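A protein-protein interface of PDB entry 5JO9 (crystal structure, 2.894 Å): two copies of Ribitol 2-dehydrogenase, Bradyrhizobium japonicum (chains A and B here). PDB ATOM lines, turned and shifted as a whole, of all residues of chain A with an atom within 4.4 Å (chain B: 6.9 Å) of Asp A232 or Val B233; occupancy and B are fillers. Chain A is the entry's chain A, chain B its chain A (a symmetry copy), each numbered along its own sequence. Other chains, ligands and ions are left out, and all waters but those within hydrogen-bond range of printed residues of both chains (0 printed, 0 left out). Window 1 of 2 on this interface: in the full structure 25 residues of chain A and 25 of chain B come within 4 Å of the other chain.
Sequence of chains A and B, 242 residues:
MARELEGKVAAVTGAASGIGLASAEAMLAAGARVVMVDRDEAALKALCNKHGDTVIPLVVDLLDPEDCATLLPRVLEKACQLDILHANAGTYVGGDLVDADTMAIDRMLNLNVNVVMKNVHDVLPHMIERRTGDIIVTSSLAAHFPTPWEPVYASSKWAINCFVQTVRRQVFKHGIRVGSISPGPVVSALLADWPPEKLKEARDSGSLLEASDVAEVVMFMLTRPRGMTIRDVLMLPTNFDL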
ATOM      1  N   HIS A 144      28.301   8.269   3.887  1.00  0.00           N
ATOM      2  CA  HIS A 144      28.688   8.685   5.230  1.00  0.00           C
ATOM      3  C   HIS A 144      29.459   7.594   5.967  1.00  0.00           C
ATOM      4  O   HIS A 144      29.478   7.578   7.201  1.00  0.00           O
ATOM      5  CB  HIS A 144      27.449   9.092   6.029  1.00  0.00           C
ATOM      6  CG  HIS A 144      26.542  10.031   5.295  1.00  0.00           C
ATOM      7  ND1 HIS A 144      26.598  11.399   5.454  1.00  0.00           N
ATOM      8  CD2 HIS A 144      25.560   9.797   4.392  1.00  0.00           C
ATOM      9  CE1 HIS A 144      25.689  11.966   4.683  1.00  0.00           C
ATOM     10  NE2 HIS A 144      25.045  11.017   4.027  1.00  0.00           N
ATOM     11  N   SER A 180      19.259  14.931  -0.982  1.00  0.00           N
ATOM     12  CA  SER A 180      19.510  13.556  -1.381  1.00  0.00           C
ATOM     13  C   SER A 180      18.958  12.613  -0.320  1.00  0.00           C
ATOM     14  O   SER A 180      18.578  13.026   0.778  1.00  0.00           O
ATOM     15  CB  SER A 180      21.008  13.303  -1.605  1.00  0.00           C
ATOM     16  OG  SER A 180      21.718  13.327  -0.380  1.00  0.00           O
ATOM     17  N   ILE A 181      18.912  11.332  -0.674  1.00  0.00           N
ATOM     18  CA  ILE A 181      18.524  10.260   0.233  1.00  0.00           C
ATOM     19  C   ILE A 181      19.693   9.291   0.327  1.00  0.00           C
ATOM     20  O   ILE A 181      20.247   8.879  -0.699  1.00  0.00           O
ATOM     21  CB  ILE A 181      17.245   9.540  -0.239  1.00  0.00           C
ATOM     22  CG1 ILE A 181      17.265   9.362  -1.763  1.00  0.00           C
ATOM     23  CG2 ILE A 181      16.006  10.305   0.223  1.00  0.00           C
ATOM     24  CD1 ILE A 181      16.066   8.625  -2.326  1.00  0.00           C
ATOM     25  N   SER A 182      20.070   8.932   1.555  1.00  0.00           N
ATOM     26  CA  SER A 182      21.218   8.067   1.818  1.00  0.00           C
ATOM     27  C   SER A 182      20.717   6.786   2.476  1.00  0.00           C
ATOM     28  O   SER A 182      20.830   6.621   3.700  1.00  0.00           O
ATOM     29  CB  SER A 182      22.248   8.775   2.696  1.00  0.00           C
ATOM     30  OG  SER A 182      22.741   9.942   2.058  1.00  0.00           O
ATOM     31  N   ILE A 230      15.152  19.954   2.975  1.00  0.00           N
ATOM     32  CA  ILE A 230      15.770  18.766   3.550  1.00  0.00           C
ATOM     33  C   ILE A 230      16.912  18.369   2.624  1.00  0.00           C
ATOM     34  O   ILE A 230      16.687  17.986   1.473  1.00  0.00           O
ATOM     35  CB  ILE A 230      14.756  17.631   3.729  1.00  0.00           C
ATOM     36  CG1 ILE A 230      13.740  18.023   4.806  1.00  0.00           C
ATOM     37  CG2 ILE A 230      15.460  16.328   4.109  1.00  0.00           C
ATOM     38  CD1 ILE A 230      12.617  17.034   4.996  1.00  0.00           C
ATOM     39  N   ARG A 231      18.140  18.471   3.126  1.00  0.00           N
ATOM     40  CA  ARG A 231      19.322  18.249   2.305  1.00  0.00           C
ATOM     41  C   ARG A 231      19.731  16.785   2.241  1.00  0.00           C
ATOM     42  O   ARG A 231      20.279  16.349   1.222  1.00  0.00           O
ATOM     43  CB  ARG A 231      20.487  19.087   2.840  1.00  0.00           C
ATOM     44  CG  ARG A 231      21.592  19.335   1.831  1.00  0.00           C
ATOM     45  CD  ARG A 231      22.589  20.357   2.350  1.00  0.00           C
ATOM     46  NE  ARG A 231      23.523  19.798   3.323  1.00  0.00           N
ATOM     47  CZ  ARG A 231      24.401  20.520   4.015  1.00  0.00           C
ATOM     48  NH1 ARG A 231      24.462  21.835   3.850  1.00  0.00           N
ATOM     49  NH2 ARG A 231      25.216  19.930   4.878  1.00  0.00           N
ATOM     50  N   ASP A 232      19.477  16.012   3.295  1.00  0.00           N
ATOM     51  CA  ASP A 232      19.837  14.601   3.297  1.00  0.00           C
ATOM     52  C   ASP A 232      18.998  13.869   4.336  1.00  0.00           C
ATOM     53  O   ASP A 232      18.512  14.465   5.301  1.00  0.00           O
ATOM     54  CB  ASP A 232      21.329  14.404   3.579  1.00  0.00           C
ATOM     55  CG  ASP A 232      21.806  13.009   3.239  1.00  0.00           C
ATOM     56  OD1 ASP A 232      21.152  12.339   2.413  1.00  0.00           O
ATOM     57  OD2 ASP A 232      22.841  12.584   3.793  1.00  0.00           O
ATOM     58  N   VAL A 233      18.837  12.563   4.121  1.00  0.00           N
ATOM     59  CA  VAL A 233      18.112  11.692   5.042  1.00  0.00           C
ATOM     60  C   VAL A 233      18.874  10.379   5.147  1.00  0.00           C
ATOM     61  O   VAL A 233      19.014   9.658   4.152  1.00  0.00           O
ATOM     62  CB  VAL A 233      16.665  11.430   4.589  1.00  0.00           C
ATOM     63  CG1 VAL A 233      15.914  10.634   5.651  1.00  0.00           C
ATOM     64  CG2 VAL A 233      15.948  12.738   4.300  1.00  0.00           C
ATOM     65  N   LEU A 234      19.361  10.064   6.346  1.00  0.00           N
ATOM     66  CA  LEU A 234      20.085   8.822   6.596  1.00  0.00           C
ATOM     67  C   LEU A 234      19.095   7.775   7.093  1.00  0.00           C
ATOM     68  O   LEU A 234      18.574   7.878   8.208  1.00  0.00           O
ATOM     69  CB  LEU A 234      21.205   9.040   7.612  1.00  0.00           C
ATOM     70  CG  LEU A 234      22.505   9.669   7.100  1.00  0.00           C
ATOM     71  CD1 LEU A 234      22.243  10.962   6.339  1.00  0.00           C
ATOM     72  CD2 LEU A 234      23.461   9.916   8.263  1.00  0.00           C
ATOM     73  N   SER B 140      22.597  19.312  14.967  1.00  0.00           N
ATOM     74  CA  SER B 140      22.525  20.585  14.267  1.00  0.00           C
ATOM     75  C   SER B 140      23.211  20.456  12.918  1.00  0.00           C
ATOM     76  O   SER B 140      23.965  19.513  12.667  1.00  0.00           O
ATOM     77  CB  SER B 140      23.174  21.709  15.076  1.00  0.00           C
ATOM     78  OG  SER B 140      23.221  22.910  14.327  1.00  0.00           O
ATOM     79  N   HIS B 144      27.641  18.771  10.577  1.00  0.00           N
ATOM     80  CA  HIS B 144      28.135  18.395   9.258  1.00  0.00           C
ATOM     81  C   HIS B 144      28.841  19.554   8.561  1.00  0.00           C
ATOM     82  O   HIS B 144      28.924  19.574   7.329  1.00  0.00           O
ATOM     83  CB  HIS B 144      26.983  17.878   8.396  1.00  0.00           C
ATOM     84  CG  HIS B 144      26.128  16.858   9.083  1.00  0.00           C
ATOM     85  ND1 HIS B 144      26.317  15.501   8.930  1.00  0.00           N
ATOM     86  CD2 HIS B 144      25.083  16.998   9.932  1.00  0.00           C
ATOM     87  CE1 HIS B 144      25.424  14.851   9.654  1.00  0.00           C
ATOM     88  NE2 HIS B 144      24.662  15.735  10.272  1.00  0.00           N
ATOM     89  N   GLY B 179      18.550   7.982  16.390  1.00  0.00           N
ATOM     90  CA  GLY B 179      18.755   8.932  15.315  1.00  0.00           C
ATOM     91  C   GLY B 179      18.869  10.329  15.880  1.00  0.00           C
ATOM     92  O   GLY B 179      18.840  10.536  17.095  1.00  0.00           O
ATOM     93  N   SER B 180      19.001  11.296  14.977  1.00  0.00           N
ATOM     94  CA  SER B 180      19.104  12.688  15.385  1.00  0.00           C
ATOM     95  C   SER B 180      18.526  13.578  14.295  1.00  0.00           C
ATOM     96  O   SER B 180      18.244  13.135  13.179  1.00  0.00           O
ATOM     97  CB  SER B 180      20.559  13.075  15.688  1.00  0.00           C
ATOM     98  OG  SER B 180      21.332  13.120  14.502  1.00  0.00           O
ATOM     99  N   ILE B 181      18.343  14.849  14.642  1.00  0.00           N
ATOM    100  CA  ILE B 181      17.908  15.884  13.713  1.00  0.00           C
ATOM    101  C   ILE B 181      18.986  16.955  13.680  1.00  0.00           C
ATOM    102  O   ILE B 181      19.444  17.413  14.732  1.00  0.00           O
ATOM    103  CB  ILE B 181      16.545  16.481  14.115  1.00  0.00           C
ATOM    104  CG1 ILE B 181      16.467  16.656  15.638  1.00  0.00           C
ATOM    105  CG2 ILE B 181      15.407  15.608  13.590  1.00  0.00           C
ATOM    106  CD1 ILE B 181      15.178  17.279  16.135  1.00  0.00           C
ATOM    107  N   SER B 182      19.394  17.350  12.472  1.00  0.00           N
ATOM    108  CA  SER B 182      20.469  18.318  12.268  1.00  0.00           C
ATOM    109  C   SER B 182      19.889  19.549  11.581  1.00  0.00           C
ATOM    110  O   SER B 182      20.051  19.726  10.364  1.00  0.00           O
ATOM    111  CB  SER B 182      21.605  17.709  11.448  1.00  0.00           C
ATOM    112  OG  SER B 182      22.169  16.591  12.114  1.00  0.00           O
ATOM    113  N   PRO B 183      19.201  20.414  12.322  1.00  0.00           N
ATOM    114  CA  PRO B 183      18.598  21.602  11.713  1.00  0.00           C
ATOM    115  C   PRO B 183      19.540  22.796  11.659  1.00  0.00           C
ATOM    116  O   PRO B 183      20.429  22.966  12.495  1.00  0.00           O
ATOM    117  CB  PRO B 183      17.413  21.890  12.644  1.00  0.00           C
ATOM    118  CG  PRO B 183      17.892  21.440  13.975  1.00  0.00           C
ATOM    119  CD  PRO B 183      18.757  20.233  13.718  1.00  0.00           C
ATOM    120  N   VAL B 217       9.156  16.602  11.440  1.00  0.00           N
ATOM    121  CA  VAL B 217      10.211  15.676  11.040  1.00  0.00           C
ATOM    122  C   VAL B 217      10.430  14.639  12.132  1.00  0.00           C
ATOM    123  O   VAL B 217      10.576  13.442  11.852  1.00  0.00           O
ATOM    124  CB  VAL B 217      11.507  16.444  10.717  1.00  0.00           C
ATOM    125  CG1 VAL B 217      12.565  15.500  10.181  1.00  0.00           C
ATOM    126  CG2 VAL B 217      11.240  17.559   9.711  1.00  0.00           C
ATOM    127  N   VAL B 218      10.441  15.078  13.392  1.00  0.00           N
ATOM    128  CA  VAL B 218      10.594  14.149  14.510  1.00  0.00           C
ATOM    129  C   VAL B 218       9.492  13.099  14.475  1.00  0.00           C
ATOM    130  O   VAL B 218       9.744  11.901  14.649  1.00  0.00           O
ATOM    131  CB  VAL B 218      10.600  14.916  15.845  1.00  0.00           C
ATOM    132  CG1 VAL B 218      10.693  13.952  17.025  1.00  0.00           C
ATOM    133  CG2 VAL B 218      11.750  15.906  15.880  1.00  0.00           C
ATOM    134  N   PHE B 220       7.773  12.149  11.821  1.00  0.00           N
ATOM    135  CA  PHE B 220       8.075  11.287  10.687  1.00  0.00           C
ATOM    136  C   PHE B 220       9.169  10.283  11.030  1.00  0.00           C
ATOM    137  O   PHE B 220       9.141   9.147  10.544  1.00  0.00           O
ATOM    138  CB  PHE B 220       8.482  12.133   9.483  1.00  0.00           C
ATOM    139  CG  PHE B 220       8.574  11.355   8.202  1.00  0.00           C
ATOM    140  CD1 PHE B 220       7.429  10.938   7.549  1.00  0.00           C
ATOM    141  CD2 PHE B 220       9.806  11.048   7.646  1.00  0.00           C
ATOM    142  CE1 PHE B 220       7.508  10.225   6.368  1.00  0.00           C
ATOM    143  CE2 PHE B 220       9.893  10.335   6.465  1.00  0.00           C
ATOM    144  CZ  PHE B 220       8.741   9.923   5.826  1.00  0.00           C
ATOM    145  N   MET B 221      10.130  10.676  11.869  1.00  0.00           N
ATOM    146  CA  MET B 221      11.150   9.734  12.321  1.00  0.00           C
ATOM    147  C   MET B 221      10.549   8.684  13.247  1.00  0.00           C
ATOM    148  O   MET B 221      10.761   7.481  13.060  1.00  0.00           O
ATOM    149  CB  MET B 221      12.285  10.484  13.023  1.00  0.00           C
ATOM    150  CG  MET B 221      13.079  11.412  12.114  1.00  0.00           C
ATOM    151  SD  MET B 221      14.369  12.313  12.996  1.00  0.00           S
ATOM    152  CE  MET B 221      15.531  10.996  13.353  1.00  0.00           C
ATOM    153  N   ILE B 230      15.587   5.927  10.820  1.00  0.00           N
ATOM    154  CA  ILE B 230      16.124   7.169  10.276  1.00  0.00           C
ATOM    155  C   ILE B 230      17.174   7.666  11.260  1.00  0.00           C
ATOM    156  O   ILE B 230      16.854   8.024  12.397  1.00  0.00           O
ATOM    157  CB  ILE B 230      15.021   8.207  10.040  1.00  0.00           C
ATOM    158  CG1 ILE B 230      14.104   7.726   8.913  1.00  0.00           C
ATOM    159  CG2 ILE B 230      15.622   9.569   9.695  1.00  0.00           C
ATOM    160  CD1 ILE B 230      12.906   8.608   8.660  1.00  0.00           C
ATOM    161  N   ARG B 231      18.431   7.679  10.824  1.00  0.00           N
ATOM    162  CA  ARG B 231      19.543   8.006  11.706  1.00  0.00           C
ATOM    163  C   ARG B 231      19.812   9.501  11.788  1.00  0.00           C
ATOM    164  O   ARG B 231      20.262   9.983  12.834  1.00  0.00           O
ATOM    165  CB  ARG B 231      20.806   7.280  11.236  1.00  0.00           C
ATOM    166  CG  ARG B 231      21.875   7.131  12.302  1.00  0.00           C
ATOM    167  CD  ARG B 231      22.987   6.206  11.840  1.00  0.00           C
ATOM    168  NE  ARG B 231      23.916   6.851  10.916  1.00  0.00           N
ATOM    169  CZ  ARG B 231      24.892   6.213  10.273  1.00  0.00           C
ATOM    170  NH1 ARG B 231      25.064   4.909  10.445  1.00  0.00           N
ATOM    171  NH2 ARG B 231      25.694   6.878   9.453  1.00  0.00           N
ATOM    172  N   ASP B 232      19.545  10.249  10.720  1.00  0.00           N
ATOM    173  CA  ASP B 232      19.773  11.687  10.734  1.00  0.00           C
ATOM    174  C   ASP B 232      18.926  12.342   9.650  1.00  0.00           C
ATOM    175  O   ASP B 232      18.550  11.706   8.662  1.00  0.00           O
ATOM    176  CB  ASP B 232      21.254  12.021  10.531  1.00  0.00           C
ATOM    177  CG  ASP B 232      21.582  13.453  10.893  1.00  0.00           C
ATOM    178  OD1 ASP B 232      20.827  14.058  11.681  1.00  0.00           O
ATOM    179  OD2 ASP B 232      22.602  13.972  10.393  1.00  0.00           O
ATOM    180  N   VAL B 233      18.635  13.628   9.853  1.00  0.00           N
ATOM    181  CA  VAL B 233      17.884  14.431   8.893  1.00  0.00           C
ATOM    182  C   VAL B 233      18.526  15.809   8.825  1.00  0.00           C
ATOM    183  O   VAL B 233      18.547  16.537   9.825  1.00  0.00           O
ATOM    184  CB  VAL B 233      16.397  14.558   9.268  1.00  0.00           C
ATOM    185  CG1 VAL B 233      15.634  15.285   8.166  1.00  0.00           C
ATOM    186  CG2 VAL B 233      15.789  13.189   9.522  1.00  0.00           C
ATOM    187  N   LEU B 234      19.046  16.169   7.653  1.00  0.00           N
ATOM    188  CA  LEU B 234      19.665  17.474   7.438  1.00  0.00           C
ATOM    189  C   LEU B 234      18.611  18.426   6.888  1.00  0.00           C
ATOM    190  O   LEU B 234      18.161  18.279   5.746  1.00  0.00           O
ATOM    191  CB  LEU B 234      20.853  17.362   6.484  1.00  0.00           C
ATOM    192  CG  LEU B 234      22.176  16.853   7.065  1.00  0.00           C
ATOM    193  CD1 LEU B 234      21.993  15.539   7.815  1.00  0.00           C
ATOM    194  CD2 LEU B 234      23.211  16.697   5.955  1.00  0.00           C
ATOM    195  N   MET B 235      18.217  19.402   7.700  1.00  0.00           N
ATOM    196  CA  MET B 235      17.245  20.411   7.309  1.00  0.00           C
ATOM    197  C   MET B 235      17.808  21.783   7.640  1.00  0.00           C
ATOM    198  O   MET B 235      18.457  21.959   8.674  1.00  0.00           O
ATOM    199  CB  MET B 235      15.905  20.195   8.023  1.00  0.00           C
ATOM    200  CG  MET B 235      15.948  20.482   9.514  1.00  0.00           C
ATOM    201  SD  MET B 235      14.555  19.780  10.410  1.00  0.00           S
ATOM    202  CE  MET B 235      15.286  18.276  11.045  1.00  0.00           C
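O of Asp A232 sits at hydrogen-bond distance from N of Leu B234 (3.0 Å). O of Leu A234 is in hydrogen-bond range of N of Arg B231, at 2.6 Å. The backbone NH (N) of Leu A234 is in hydrogen-bond range of the backbone carbonyl oxygen (O) of Asp B232, at 3.0 Å. The backbone carbonyl oxygen (O) of Leu B234 sits at hydrogen-bond distance from the backbone NH (N) of Arg A231.
Of the printed residues of chain B, Ile A230 touches Leu B234. Of chain B, only Val B233 and Leu B234 come within 4 Å of Asp A232. Of the printed residues of chain B, Leu A234 touches Ile B230 (3.3 Å), Arg B231 (2.6 Å) and Asp B232 (3.0 Å). Of the printed residues of chain A, Arg B231 touches Leu A234. Of chain A, only Asp A232 comes within 4 Å of Val B233. The nearest residue of chain A that does not touch Val B233 is Ile A230 (4.2 Å).
Ile A230 touches Leu B234, and with the chains exchanged Leu A234 touches Ile B230. Arg A231 touches Leu B234, and with the chains exchanged Leu A234 touches Arg B231. Asp A232 touches Val B233, and with the chains exchanged Val A233 touches Asp B232. Asp A232 touches Leu B234, and with the chains exchanged Leu A234 touches Asp B232. Positions printed for both chains: 144, 180, 181, 182, 230, 231, 232, 233 and 234. Of the 8 pairs that touch across the chains among the printed residues, 8 have their exchanged pair printed and touching as well.
Among the printed residues, merely in contact across the chains: Ile A230 with Leu B234, Leu A234 with Ile B230, Val A233 with Asp B232 and Asp A232 with Val B233.
Printed residues of chain A that touch a printed residue of chain B: Ile A230, Arg A231, Asp A232, Val A233 and Leu A234. Hydrophobic or aromatic side chains of chain A that line the printed part of chain B: Ile A230 and Leu A234. Of the 17 printed residues of chain B, 5 touch a printed residue of chain A. Printed residues of chain B that touch a printed residue of chain A: Ile B230, Arg B231, Asp B232, Val B233 and Leu B234. Hydrophobic or aromatic side chains of chain B within 4 Å of the printed part of chain A: Ile B230 and Leu B234. Among the printed residues, 8 pairs touch across the chains. Among the printed residues, no Asp or Glu carboxylate lies within 4 Å of a Lys or Arg side-chain nitrogen of the other chain.
The side-chain hydroxyl of Ser B180 sits at hydrogen-bond distance from the side-chain carboxylate of Asp B232 (3.0 Å). The backbone NH (N) of Ser B180 lies within hydrogen-bond range of the backbone carbonyl oxygen (O) of Arg B231 (2.8 Å). The backbone carbonyl oxygen of Val A233 is in hydrogen-bond range of the backbone NH of Ser A182, at 2.9 Å. The side-chain carboxylate (OD2) of Asp A232 sits at hydrogen-bond distance from a ring nitrogen (NE2) of His A144 (2.7 Å). O of Ser B180 sits at hydrogen-bond distance from N of Val B233, 3.4 Å away. The side-chain hydroxyl (OG) of Ser A180 sits at hydrogen-bond distance from the side-chain carboxylate (OD1) of Asp A232 (3.0 Å).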
